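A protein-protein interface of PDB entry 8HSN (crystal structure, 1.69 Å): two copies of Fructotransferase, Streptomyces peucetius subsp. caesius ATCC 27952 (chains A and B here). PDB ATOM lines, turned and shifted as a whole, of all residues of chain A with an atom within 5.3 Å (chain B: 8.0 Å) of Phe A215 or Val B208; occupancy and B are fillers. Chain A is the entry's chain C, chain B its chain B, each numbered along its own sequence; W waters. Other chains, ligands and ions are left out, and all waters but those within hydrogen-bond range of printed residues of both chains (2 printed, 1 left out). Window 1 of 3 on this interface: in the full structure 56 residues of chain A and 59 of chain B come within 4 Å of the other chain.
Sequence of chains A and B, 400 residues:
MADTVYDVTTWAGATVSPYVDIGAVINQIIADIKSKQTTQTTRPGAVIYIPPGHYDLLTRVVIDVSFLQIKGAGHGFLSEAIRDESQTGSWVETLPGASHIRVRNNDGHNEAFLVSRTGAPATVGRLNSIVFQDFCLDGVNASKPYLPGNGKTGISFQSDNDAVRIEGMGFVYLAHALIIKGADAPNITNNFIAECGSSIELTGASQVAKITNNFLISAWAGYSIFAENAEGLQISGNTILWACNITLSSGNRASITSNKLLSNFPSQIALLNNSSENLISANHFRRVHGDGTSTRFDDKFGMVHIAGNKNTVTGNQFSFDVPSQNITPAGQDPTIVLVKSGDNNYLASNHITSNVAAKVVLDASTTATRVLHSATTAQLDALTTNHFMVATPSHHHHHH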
ATOM      1  N   ASN A 191       2.543   3.535 -21.007  1.00  0.00           N
ATOM      2  CA  ASN A 191       2.268   4.804 -21.660  1.00  0.00           C
ATOM      3  C   ASN A 191       3.493   5.309 -22.423  1.00  0.00           C
ATOM      4  O   ASN A 191       4.604   4.809 -22.267  1.00  0.00           O
ATOM      5  CB  ASN A 191       1.832   5.846 -20.627  1.00  0.00           C
ATOM      6  CG  ASN A 191       0.585   5.420 -19.883  1.00  0.00           C
ATOM      7  OD1 ASN A 191      -0.505   5.380 -20.447  1.00  0.00           O
ATOM      8  ND2 ASN A 191       0.739   5.094 -18.607  1.00  0.00           N
ATOM      9  N   PHE A 192       3.261   6.308 -23.271  1.00  0.00           N
ATOM     10  CA  PHE A 192       4.304   6.980 -24.046  1.00  0.00           C
ATOM     11  C   PHE A 192       4.129   8.474 -23.784  1.00  0.00           C
ATOM     12  O   PHE A 192       3.246   9.105 -24.382  1.00  0.00           O
ATOM     13  CB  PHE A 192       4.202   6.656 -25.552  1.00  0.00           C
ATOM     14  CG  PHE A 192       5.465   6.929 -26.311  1.00  0.00           C
ATOM     15  CD1 PHE A 192       5.817   8.232 -26.651  1.00  0.00           C
ATOM     16  CD2 PHE A 192       6.319   5.891 -26.673  1.00  0.00           C
ATOM     17  CE1 PHE A 192       7.006   8.494 -27.287  1.00  0.00           C
ATOM     18  CE2 PHE A 192       7.519   6.152 -27.332  1.00  0.00           C
ATOM     19  CZ  PHE A 192       7.847   7.458 -27.653  1.00  0.00           C
ATOM     20  N   ILE A 193       4.913   9.017 -22.851  1.00  0.00           N
ATOM     21  CA  ILE A 193       4.835  10.426 -22.466  1.00  0.00           C
ATOM     22  C   ILE A 193       6.126  11.093 -22.906  1.00  0.00           C
ATOM     23  O   ILE A 193       7.211  10.709 -22.461  1.00  0.00           O
ATOM     24  CB  ILE A 193       4.615  10.591 -20.950  1.00  0.00           C
ATOM     25  CG1 ILE A 193       3.316   9.920 -20.551  1.00  0.00           C
ATOM     26  CG2 ILE A 193       4.626  12.079 -20.587  1.00  0.00           C
ATOM     27  CD1 ILE A 193       3.111   9.834 -19.053  1.00  0.00           C
ATOM     28  N   ALA A 194       6.031  12.077 -23.791  1.00  0.00           N
ATOM     29  CA  ALA A 194       7.251  12.641 -24.342  1.00  0.00           C
ATOM     30  C   ALA A 194       7.044  14.106 -24.681  1.00  0.00           C
ATOM     31  O   ALA A 194       5.941  14.525 -25.029  1.00  0.00           O
ATOM     32  CB  ALA A 194       7.706  11.861 -25.586  1.00  0.00           C
ATOM     33  N   ASN A 213       6.648   0.057 -17.014  1.00  0.00           N
ATOM     34  CA  ASN A 213       6.635  -0.242 -18.445  1.00  0.00           C
ATOM     35  C   ASN A 213       6.252   0.965 -19.291  1.00  0.00           C
ATOM     36  O   ASN A 213       5.667   0.811 -20.365  1.00  0.00           O
ATOM     37  CB  ASN A 213       5.678  -1.401 -18.718  1.00  0.00           C
ATOM     38  CG  ASN A 213       5.850  -1.996 -20.091  1.00  0.00           C
ATOM     39  OD1 ASN A 213       6.949  -1.973 -20.671  1.00  0.00           O
ATOM     40  ND2 ASN A 213       4.765  -2.526 -20.627  1.00  0.00           N
ATOM     41  N   ASN A 214       6.623   2.163 -18.847  1.00  0.00           N
ATOM     42  CA  ASN A 214       6.373   3.397 -19.583  1.00  0.00           C
ATOM     43  C   ASN A 214       7.625   3.894 -20.303  1.00  0.00           C
ATOM     44  O   ASN A 214       8.755   3.663 -19.868  1.00  0.00           O
ATOM     45  CB  ASN A 214       5.928   4.523 -18.642  1.00  0.00           C
ATOM     46  CG  ASN A 214       4.675   4.175 -17.872  1.00  0.00           C
ATOM     47  OD1 ASN A 214       3.559   4.168 -18.420  1.00  0.00           O
ATOM     48  ND2 ASN A 214       4.843   3.933 -16.575  1.00  0.00           N
ATOM     49  N   PHE A 215       7.406   4.629 -21.392  1.00  0.00           N
ATOM     50  CA  PHE A 215       8.378   5.603 -21.876  1.00  0.00           C
ATOM     51  C   PHE A 215       8.040   6.956 -21.240  1.00  0.00           C
ATOM     52  O   PHE A 215       6.911   7.457 -21.406  1.00  0.00           O
ATOM     53  CB  PHE A 215       8.315   5.750 -23.394  1.00  0.00           C
ATOM     54  CG  PHE A 215       9.030   4.674 -24.177  1.00  0.00           C
ATOM     55  CD1 PHE A 215      10.420   4.686 -24.304  1.00  0.00           C
ATOM     56  CD2 PHE A 215       8.314   3.683 -24.823  1.00  0.00           C
ATOM     57  CE1 PHE A 215      11.070   3.718 -25.050  1.00  0.00           C
ATOM     58  CE2 PHE A 215       8.962   2.718 -25.570  1.00  0.00           C
ATOM     59  CZ  PHE A 215      10.328   2.723 -25.668  1.00  0.00           C
ATOM     60  N   LEU A 216       8.996   7.552 -20.526  1.00  0.00           N
ATOM     61  CA  LEU A 216       8.838   8.879 -19.932  1.00  0.00           C
ATOM     62  C   LEU A 216       9.975   9.755 -20.444  1.00  0.00           C
ATOM     63  O   LEU A 216      11.141   9.482 -20.157  1.00  0.00           O
ATOM     64  CB  LEU A 216       8.847   8.830 -18.403  1.00  0.00           C
ATOM     65  CG  LEU A 216       7.901   7.825 -17.765  1.00  0.00           C
ATOM     66  CD1 LEU A 216       8.091   7.804 -16.251  1.00  0.00           C
ATOM     67  CD2 LEU A 216       6.473   8.163 -18.098  1.00  0.00           C
ATOM     68  N   ILE A 217       9.630  10.786 -21.217  1.00  0.00           N
ATOM     69  CA  ILE A 217      10.598  11.580 -21.977  1.00  0.00           C
ATOM     70  C   ILE A 217      10.299  13.071 -21.829  1.00  0.00           C
ATOM     71  O   ILE A 217      10.200  13.797 -22.829  1.00  0.00           O
ATOM     72  CB  ILE A 217      10.666  11.145 -23.453  1.00  0.00           C
ATOM     73  CG1 ILE A 217      10.621   9.617 -23.539  1.00  0.00           C
ATOM     74  CG2 ILE A 217      11.949  11.699 -24.072  1.00  0.00           C
ATOM     75  CD1 ILE A 217      10.670   9.053 -24.953  1.00  0.00           C
ATOM     76  N   THR A 239      11.482   3.061 -19.282  1.00  0.00           N
ATOM     77  CA  THR A 239      12.559   3.728 -20.013  1.00  0.00           C
ATOM     78  C   THR A 239      12.315   5.222 -19.888  1.00  0.00           C
ATOM     79  O   THR A 239      11.320   5.743 -20.418  1.00  0.00           O
ATOM     80  CB  THR A 239      12.594   3.268 -21.463  1.00  0.00           C
ATOM     81  OG1 THR A 239      13.024   1.904 -21.508  1.00  0.00           O
ATOM     82  CG2 THR A 239      13.585   4.120 -22.265  1.00  0.00           C
ATOM     83  N   LEU A 241      13.962   9.000 -20.229  1.00  0.00           N
ATOM     84  CA  LEU A 241      14.972   9.545 -21.113  1.00  0.00           C
ATOM     85  C   LEU A 241      14.970  11.071 -21.116  1.00  0.00           C
ATOM     86  O   LEU A 241      14.129  11.721 -20.485  1.00  0.00           O
ATOM     87  CB  LEU A 241      14.771   9.064 -22.558  1.00  0.00           C
ATOM     88  CG  LEU A 241      14.625   7.556 -22.722  1.00  0.00           C
ATOM     89  CD1 LEU A 241      14.167   7.183 -24.137  1.00  0.00           C
ATOM     90  CD2 LEU A 241      15.945   6.866 -22.395  1.00  0.00           C
ATOM     91  N   LYS A 260      15.582   1.627 -17.157  1.00  0.00           N
ATOM     92  CA  LYS A 260      16.586   2.263 -18.008  1.00  0.00           C
ATOM     93  C   LYS A 260      16.436   3.770 -17.832  1.00  0.00           C
ATOM     94  O   LYS A 260      15.394   4.334 -18.176  1.00  0.00           O
ATOM     95  CB  LYS A 260      16.339   1.809 -19.446  1.00  0.00           C
ATOM     96  CG  LYS A 260      16.861   2.703 -20.546  1.00  0.00           C
ATOM     97  CD  LYS A 260      18.304   2.645 -20.632  1.00  0.00           C
ATOM     98  CE  LYS A 260      18.822   3.681 -21.645  1.00  0.00           C
ATOM     99  NZ  LYS A 260      20.297   3.700 -21.609  1.00  0.00           N
ATOM    100  N   ASP B 162       9.276   5.248 -35.447  1.00  0.00           N
ATOM    101  CA  ASP B 162       9.288   5.819 -34.104  1.00  0.00           C
ATOM    102  C   ASP B 162       8.041   5.394 -33.335  1.00  0.00           C
ATOM    103  O   ASP B 162       6.919   5.467 -33.843  1.00  0.00           O
ATOM    104  CB  ASP B 162       9.371   7.347 -34.162  1.00  0.00           C
ATOM    105  CG  ASP B 162       9.704   7.969 -32.833  1.00  0.00           C
ATOM    106  OD1 ASP B 162      10.531   7.410 -32.079  1.00  0.00           O
ATOM    107  OD2 ASP B 162       9.138   9.037 -32.546  1.00  0.00           O
ATOM    108  N   ALA B 163       8.255   4.933 -32.106  1.00  0.00           N
ATOM    109  CA  ALA B 163       7.198   4.643 -31.141  1.00  0.00           C
ATOM    110  C   ALA B 163       6.227   3.569 -31.633  1.00  0.00           C
ATOM    111  O   ALA B 163       5.043   3.584 -31.279  1.00  0.00           O
ATOM    112  CB  ALA B 163       6.456   5.925 -30.754  1.00  0.00           C
ATOM    113  N   VAL B 164       6.706   2.593 -32.415  1.00  0.00           N
ATOM    114  CA  VAL B 164       5.817   1.515 -32.841  1.00  0.00           C
ATOM    115  C   VAL B 164       5.554   0.620 -31.636  1.00  0.00           C
ATOM    116  O   VAL B 164       6.260   0.699 -30.620  1.00  0.00           O
ATOM    117  CB  VAL B 164       6.344   0.699 -34.032  1.00  0.00           C
ATOM    118  CG1 VAL B 164       6.662   1.629 -35.199  1.00  0.00           C
ATOM    119  CG2 VAL B 164       7.565  -0.138 -33.675  1.00  0.00           C
ATOM    120  N   ARG B 165       4.549  -0.238 -31.753  1.00  0.00           N
ATOM    121  CA  ARG B 165       4.022  -0.975 -30.604  1.00  0.00           C
ATOM    122  C   ARG B 165       3.498  -2.326 -31.062  1.00  0.00           C
ATOM    123  O   ARG B 165       2.615  -2.410 -31.925  1.00  0.00           O
ATOM    124  CB  ARG B 165       2.926  -0.149 -29.955  1.00  0.00           C
ATOM    125  CG  ARG B 165       2.237  -0.723 -28.742  1.00  0.00           C
ATOM    126  CD  ARG B 165       1.311   0.344 -28.179  1.00  0.00           C
ATOM    127  NE  ARG B 165       0.378  -0.146 -27.174  1.00  0.00           N
ATOM    128  CZ  ARG B 165      -0.577   0.599 -26.641  1.00  0.00           C
ATOM    129  NH1 ARG B 165      -0.736   1.866 -26.986  1.00  0.00           N
ATOM    130  NH2 ARG B 165      -1.383   0.065 -25.733  1.00  0.00           N
ATOM    131  N   ALA B 183      14.688   1.169 -35.630  1.00  0.00           N
ATOM    132  CA  ALA B 183      13.626   1.449 -34.682  1.00  0.00           C
ATOM    133  C   ALA B 183      14.060   2.460 -33.625  1.00  0.00           C
ATOM    134  O   ALA B 183      15.120   2.320 -33.005  1.00  0.00           O
ATOM    135  CB  ALA B 183      13.197   0.162 -33.988  1.00  0.00           C
ATOM    136  N   ASP B 184      13.205   3.442 -33.382  1.00  0.00           N
ATOM    137  CA  ASP B 184      13.374   4.434 -32.332  1.00  0.00           C
ATOM    138  C   ASP B 184      12.212   4.270 -31.358  1.00  0.00           C
ATOM    139  O   ASP B 184      11.046   4.342 -31.765  1.00  0.00           O
ATOM    140  CB  ASP B 184      13.399   5.828 -32.958  1.00  0.00           C
ATOM    141  CG  ASP B 184      13.925   6.876 -32.051  1.00  0.00           C
ATOM    142  OD1 ASP B 184      14.205   6.591 -30.863  1.00  0.00           O
ATOM    143  OD2 ASP B 184      14.050   8.032 -32.540  1.00  0.00           O
ATOM    144  N   ALA B 185      12.541   3.987 -30.094  1.00  0.00           N
ATOM    145  CA  ALA B 185      11.568   3.776 -29.030  1.00  0.00           C
ATOM    146  C   ALA B 185      10.429   2.815 -29.381  1.00  0.00           C
ATOM    147  O   ALA B 185       9.268   3.086 -29.068  1.00  0.00           O
ATOM    148  CB  ALA B 185      11.003   5.119 -28.583  1.00  0.00           C
ATOM    149  N   PRO B 186      10.730   1.659 -29.988  1.00  0.00           N
ATOM    150  CA  PRO B 186       9.690   0.637 -30.154  1.00  0.00           C
ATOM    151  C   PRO B 186       9.314   0.026 -28.812  1.00  0.00           C
ATOM    152  O   PRO B 186      10.115  -0.020 -27.882  1.00  0.00           O
ATOM    153  CB  PRO B 186      10.356  -0.401 -31.053  1.00  0.00           C
ATOM    154  CG  PRO B 186      11.783  -0.308 -30.643  1.00  0.00           C
ATOM    155  CD  PRO B 186      12.035   1.156 -30.446  1.00  0.00           C
ATOM    156  N   ASN B 187       8.078  -0.440 -28.728  1.00  0.00           N
ATOM    157  CA  ASN B 187       7.527  -1.066 -27.530  1.00  0.00           C
ATOM    158  C   ASN B 187       7.080  -2.469 -27.909  1.00  0.00           C
ATOM    159  O   ASN B 187       6.123  -2.624 -28.674  1.00  0.00           O
ATOM    160  CB  ASN B 187       6.367  -0.232 -27.008  1.00  0.00           C
ATOM    161  CG  ASN B 187       5.773  -0.788 -25.754  1.00  0.00           C
ATOM    162  OD1 ASN B 187       6.418  -1.540 -25.022  1.00  0.00           O
ATOM    163  ND2 ASN B 187       4.545  -0.415 -25.489  1.00  0.00           N
ATOM    164  N   ILE B 188       7.788  -3.487 -27.411  1.00  0.00           N
ATOM    165  CA  ILE B 188       7.499  -4.886 -27.726  1.00  0.00           C
ATOM    166  C   ILE B 188       7.149  -5.547 -26.396  1.00  0.00           C
ATOM    167  O   ILE B 188       8.043  -5.873 -25.604  1.00  0.00           O
ATOM    168  CB  ILE B 188       8.672  -5.581 -28.416  1.00  0.00           C
ATOM    169  CG1 ILE B 188       9.098  -4.809 -29.682  1.00  0.00           C
ATOM    170  CG2 ILE B 188       8.325  -7.006 -28.807  1.00  0.00           C
ATOM    171  CD1 ILE B 188      10.444  -5.209 -30.213  1.00  0.00           C
ATOM    172  N   LEU B 202      16.267  -6.574 -33.973  1.00  0.00           N
ATOM    173  CA  LEU B 202      16.326  -5.126 -34.179  1.00  0.00           C
ATOM    174  C   LEU B 202      17.561  -4.847 -35.024  1.00  0.00           C
ATOM    175  O   LEU B 202      18.684  -4.770 -34.515  1.00  0.00           O
ATOM    176  CB  LEU B 202      16.376  -4.379 -32.857  1.00  0.00           C
ATOM    177  CG  LEU B 202      15.231  -4.734 -31.916  1.00  0.00           C
ATOM    178  CD1 LEU B 202      15.517  -4.014 -30.610  1.00  0.00           C
ATOM    179  CD2 LEU B 202      13.915  -4.324 -32.505  1.00  0.00           C
ATOM    180  N   ALA B 205      20.074  -0.328 -36.901  1.00  0.00           N
ATOM    181  CA  ALA B 205      20.409   0.377 -35.674  1.00  0.00           C
ATOM    182  C   ALA B 205      19.106   0.546 -34.916  1.00  0.00           C
ATOM    183  O   ALA B 205      18.023   0.439 -35.499  1.00  0.00           O
ATOM    184  CB  ALA B 205      21.053   1.736 -35.947  1.00  0.00           C
ATOM    185  N   SER B 206      19.209   0.846 -33.621  1.00  0.00           N
ATOM    186  CA  SER B 206      18.020   1.169 -32.853  1.00  0.00           C
ATOM    187  C   SER B 206      18.393   2.095 -31.709  1.00  0.00           C
ATOM    188  O   SER B 206      19.549   2.159 -31.279  1.00  0.00           O
ATOM    189  CB  SER B 206      17.330  -0.094 -32.313  1.00  0.00           C
ATOM    190  OG  SER B 206      18.125  -0.732 -31.323  1.00  0.00           O
ATOM    191  N   GLN B 207      17.384   2.817 -31.231  1.00  0.00           N
ATOM    192  CA  GLN B 207      17.471   3.642 -30.039  1.00  0.00           C
ATOM    193  C   GLN B 207      16.342   3.272 -29.091  1.00  0.00           C
ATOM    194  O   GLN B 207      15.173   3.204 -29.501  1.00  0.00           O
ATOM    195  CB  GLN B 207      17.398   5.139 -30.381  1.00  0.00           C
ATOM    196  CG  GLN B 207      18.754   5.704 -30.851  1.00  0.00           C
ATOM    197  CD  GLN B 207      19.630   6.267 -29.703  1.00  0.00           C
ATOM    198  OE1 GLN B 207      19.329   6.118 -28.493  1.00  0.00           O
ATOM    199  NE2 GLN B 207      20.741   6.893 -30.086  1.00  0.00           N
ATOM    200  N   VAL B 208      16.714   3.040 -27.827  1.00  0.00           N
ATOM    201  CA  VAL B 208      15.838   2.859 -26.665  1.00  0.00           C
ATOM    202  C   VAL B 208      14.623   1.982 -26.938  1.00  0.00           C
ATOM    203  O   VAL B 208      13.493   2.302 -26.547  1.00  0.00           O
ATOM    204  CB  VAL B 208      15.447   4.241 -26.085  1.00  0.00           C
ATOM    205  CG1 VAL B 208      16.686   4.966 -25.575  1.00  0.00           C
ATOM    206  CG2 VAL B 208      14.738   5.103 -27.111  1.00  0.00           C
ATOM    207  N   ALA B 209      14.861   0.817 -27.534  1.00  0.00           N
ATOM    208  CA  ALA B 209      13.831  -0.203 -27.621  1.00  0.00           C
ATOM    209  C   ALA B 209      13.466  -0.699 -26.225  1.00  0.00           C
ATOM    210  O   ALA B 209      14.322  -0.820 -25.350  1.00  0.00           O
ATOM    211  CB  ALA B 209      14.324  -1.367 -28.476  1.00  0.00           C
ATOM    212  N   LYS B 210      12.186  -0.983 -26.029  1.00  0.00           N
ATOM    213  CA  LYS B 210      11.662  -1.493 -24.775  1.00  0.00           C
ATOM    214  C   LYS B 210      11.050  -2.851 -25.071  1.00  0.00           C
ATOM    215  O   LYS B 210      10.078  -2.937 -25.830  1.00  0.00           O
ATOM    216  CB  LYS B 210      10.627  -0.539 -24.174  1.00  0.00           C
ATOM    217  CG  LYS B 210       9.992  -1.063 -22.887  1.00  0.00           C
ATOM    218  CD  LYS B 210       9.486   0.027 -21.936  1.00  0.00           C
ATOM    219  CE  LYS B 210       8.330   0.827 -22.494  1.00  0.00           C
ATOM    220  NZ  LYS B 210       7.086   0.035 -22.703  1.00  0.00           N
ATOM    221  N   ILE B 211      11.636  -3.907 -24.490  1.00  0.00           N
ATOM    222  CA  ILE B 211      11.208  -5.288 -24.706  1.00  0.00           C
ATOM    223  C   ILE B 211      10.875  -5.843 -23.328  1.00  0.00           C
ATOM    224  O   ILE B 211      11.780  -6.186 -22.556  1.00  0.00           O
ATOM    225  CB  ILE B 211      12.279  -6.139 -25.395  1.00  0.00           C
ATOM    226  CG1 ILE B 211      12.672  -5.524 -26.752  1.00  0.00           C
ATOM    227  CG2 ILE B 211      11.780  -7.585 -25.548  1.00  0.00           C
ATOM    228  CD1 ILE B 211      13.858  -6.222 -27.432  1.00  0.00           C
ATOM    229  N   ASN B 229      23.992  -2.229 -33.400  1.00  0.00           N
ATOM    230  CA  ASN B 229      24.078  -0.773 -33.310  1.00  0.00           C
ATOM    231  C   ASN B 229      22.918  -0.230 -32.482  1.00  0.00           C
ATOM    232  O   ASN B 229      22.193   0.678 -32.881  1.00  0.00           O
ATOM    233  CB  ASN B 229      24.116  -0.155 -34.713  1.00  0.00           C
ATOM    234  CG  ASN B 229      25.250  -0.703 -35.555  1.00  0.00           C
ATOM    235  OD1 ASN B 229      26.390  -0.792 -35.104  1.00  0.00           O
ATOM    236  ND2 ASN B 229      24.943  -1.077 -36.786  1.00  0.00           N
ATOM    237  N   ALA B 230      22.730  -0.840 -31.315  1.00  0.00           N
ATOM    238  CA  ALA B 230      21.573  -0.609 -30.467  1.00  0.00           C
ATOM    239  C   ALA B 230      21.998   0.166 -29.236  1.00  0.00           C
ATOM    240  O   ALA B 230      22.783  -0.333 -28.411  1.00  0.00           O
ATOM    241  CB  ALA B 230      20.941  -1.938 -30.062  1.00  0.00           C
ATOM    242  N   GLU B 231      21.486   1.380 -29.115  1.00  0.00           N
ATOM    243  CA  GLU B 231      21.727   2.235 -27.957  1.00  0.00           C
ATOM    244  C   GLU B 231      20.544   2.146 -27.003  1.00  0.00           C
ATOM    245  O   GLU B 231      19.403   2.330 -27.419  1.00  0.00           O
ATOM    246  CB  GLU B 231      21.943   3.686 -28.390  1.00  0.00           C
ATOM    247  CG  GLU B 231      22.171   4.656 -27.247  1.00  0.00           C
ATOM    248  CD  GLU B 231      23.516   4.482 -26.548  1.00  0.00           C
ATOM    249  OE1 GLU B 231      24.503   4.034 -27.176  1.00  0.00           O
ATOM    250  OE2 GLU B 231      23.609   4.788 -25.338  1.00  0.00           O
ATOM    251  N   GLY B 232      20.828   1.872 -25.721  1.00  0.00           N
ATOM    252  CA  GLY B 232      19.827   2.038 -24.667  1.00  0.00           C
ATOM    253  C   GLY B 232      18.697   1.036 -24.631  1.00  0.00           C
ATOM    254  O   GLY B 232      17.604   1.364 -24.155  1.00  0.00           O
ATOM    255  N   LEU B 233      18.925  -0.177 -25.124  1.00  0.00           N
ATOM    256  CA  LEU B 233      17.924  -1.231 -25.061  1.00  0.00           C
ATOM    257  C   LEU B 233      17.499  -1.500 -23.621  1.00  0.00           C
ATOM    258  O   LEU B 233      18.320  -1.535 -22.707  1.00  0.00           O
ATOM    259  CB  LEU B 233      18.524  -2.501 -25.674  1.00  0.00           C
ATOM    260  CG  LEU B 233      17.902  -3.354 -26.760  1.00  0.00           C
ATOM    261  CD1 LEU B 233      18.815  -4.595 -26.883  1.00  0.00           C
ATOM    262  CD2 LEU B 233      16.485  -3.703 -26.417  1.00  0.00           C
ATOM    263  N   GLN B 234      16.207  -1.707 -23.411  1.00  0.00           N
ATOM    264  CA  GLN B 234      15.696  -2.163 -22.130  1.00  0.00           C
ATOM    265  C   GLN B 234      14.998  -3.495 -22.319  1.00  0.00           C
ATOM    266  O   GLN B 234      14.040  -3.585 -23.093  1.00  0.00           O
ATOM    267  CB  GLN B 234      14.748  -1.161 -21.499  1.00  0.00           C
ATOM    268  CG  GLN B 234      14.615  -1.503 -20.026  1.00  0.00           C
ATOM    269  CD  GLN B 234      13.251  -1.336 -19.433  1.00  0.00           C
ATOM    270  OE1 GLN B 234      12.361  -0.636 -19.952  1.00  0.00           O
ATOM    271  NE2 GLN B 234      13.043  -2.028 -18.343  1.00  0.00           N
ATOM    272  N   ASN B 252      25.162  -0.778 -26.758  1.00  0.00           N
ATOM    273  CA  ASN B 252      25.708  -0.084 -25.593  1.00  0.00           C
ATOM    274  C   ASN B 252      24.598   0.479 -24.715  1.00  0.00           C
ATOM    275  O   ASN B 252      23.526   0.844 -25.196  1.00  0.00           O
ATOM    276  CB  ASN B 252      26.627   1.076 -25.988  1.00  0.00           C
ATOM    277  CG  ASN B 252      27.744   0.641 -26.896  1.00  0.00           C
ATOM    278  OD1 ASN B 252      28.765   0.108 -26.437  1.00  0.00           O
ATOM    279  ND2 ASN B 252      27.561   0.850 -28.188  1.00  0.00           N
ATOM    280  N   ARG B 253      24.894   0.573 -23.418  1.00  0.00           N
ATOM    281  CA  ARG B 253      24.006   1.193 -22.426  1.00  0.00           C
ATOM    282  C   ARG B 253      22.653   0.482 -22.341  1.00  0.00           C
ATOM    283  O   ARG B 253      21.630   1.107 -22.028  1.00  0.00           O
ATOM    284  CB  ARG B 253      23.821   2.685 -22.712  1.00  0.00           C
ATOM    285  CG  ARG B 253      24.879   3.596 -22.107  1.00  0.00           C
ATOM    286  CD  ARG B 253      26.203   3.520 -22.790  1.00  0.00           C
ATOM    287  NE  ARG B 253      26.163   4.024 -24.159  1.00  0.00           N
ATOM    288  CZ  ARG B 253      27.247   4.226 -24.888  1.00  0.00           C
ATOM    289  NH1 ARG B 253      28.445   4.068 -24.374  1.00  0.00           N
ATOM    290  NH2 ARG B 253      27.121   4.566 -26.169  1.00  0.00           N
HETATM  291  O   HOH W   1      21.258   4.981 -23.809  1.00  0.00           O
HETATM  292  O   HOH W   2       5.299   2.105 -23.477  1.00  0.00           O
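No position is printed for both chains. Of the 13 pairs that touch across the chains among the printed residues, none has its exchanged pair printed and touching as well.
Water W1 bridges NZ of Lys A260 (2.7 Å) and OE2 of Glu B231 (2.8 Å). Water W2 lies within hydrogen-bond range of the side-chain amino group of Lys B210, the backbone carbonyl oxygen of Asn A191, the side-chain amide nitrogen of Asn B187 and the backbone carbonyl oxygen of Asn A213.
Among the printed residues, merely in contact across the chains: Phe A215 with Val B208 (3.2 Å), Lys A260 with Gly B232 (3.5 Å), Phe A215 with Ala B185 (3.5 Å), Phe A215 with Pro B186 (3.5 Å), Phe A192 with Ala B163 (3.6 Å), Phe A215 with Lys B210 (3.6 Å), Leu A241 with Val B208 (3.7 Å), Lys A260 with Gln B234 (3.8 Å), Asn A214 with Lys B210 (3.8 Å) and Phe A192 with Ala B185 (3.8 Å).
The side-chain amino group of Lys B210 lies within hydrogen-bond range of the backbone carbonyl oxygen of Asn A213 (2.8 Å). The side-chain hydroxyl (OG1) of Thr A239 sits at hydrogen-bond distance from the side-chain amide oxygen (OE1) of Gln B234, at 3.1 Å. The side-chain amino group (NZ) of Lys A260 sits at hydrogen-bond distance from the backbone carbonyl oxygen (O) of Arg B253 (2.9 Å).
Printed residues of chain B that touch a printed residue of chain A: Ala B163, Ala B185, Pro B186, Val B208, Lys B210, Gly B232, Gln B234 and Arg B253. Among the printed residues, no Asp or Glu carboxylate lies within 4 Å of a Lys or Arg side-chain nitrogen of the other chain.
The backbone NH of Ala B185 is in hydrogen-bond range of the backbone carbonyl oxygen of Gln B207. The backbone carbonyl oxygen of Pro B186 sits at hydrogen-bond distance from the backbone NH of Lys B210 (2.9 Å). N of Ile B188 is in hydrogen-bond range of O of Lys B210 (2.8 Å). N of Gly B232 lies within hydrogen-bond range of O of Asn B252. The side-chain amide oxygen (OD1) of Asn A214 lies within hydrogen-bond range of the backbone NH (N) of Asn A191 (2.9 Å). The backbone NH (N) of Thr A239 sits at hydrogen-bond distance from the backbone carbonyl oxygen (O) of Asn A214, 2.9 Å away.
Printed residues of chain B within 4 Å of Asn A213: Lys B210. Of the printed residues of chain B, Asn A214 touches Lys B210 (3.8 Å). Phe A215 touches four residues of chain B. Of chain A, only Phe A215 and Leu A241 come within 4 Å of Val B208. The nearest residue of chain B that does not touch Phe A215 is Asn B187 (4.2 Å). The nearest residue of chain A that does not touch Val B208 is Thr A239 (4.3 Å).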
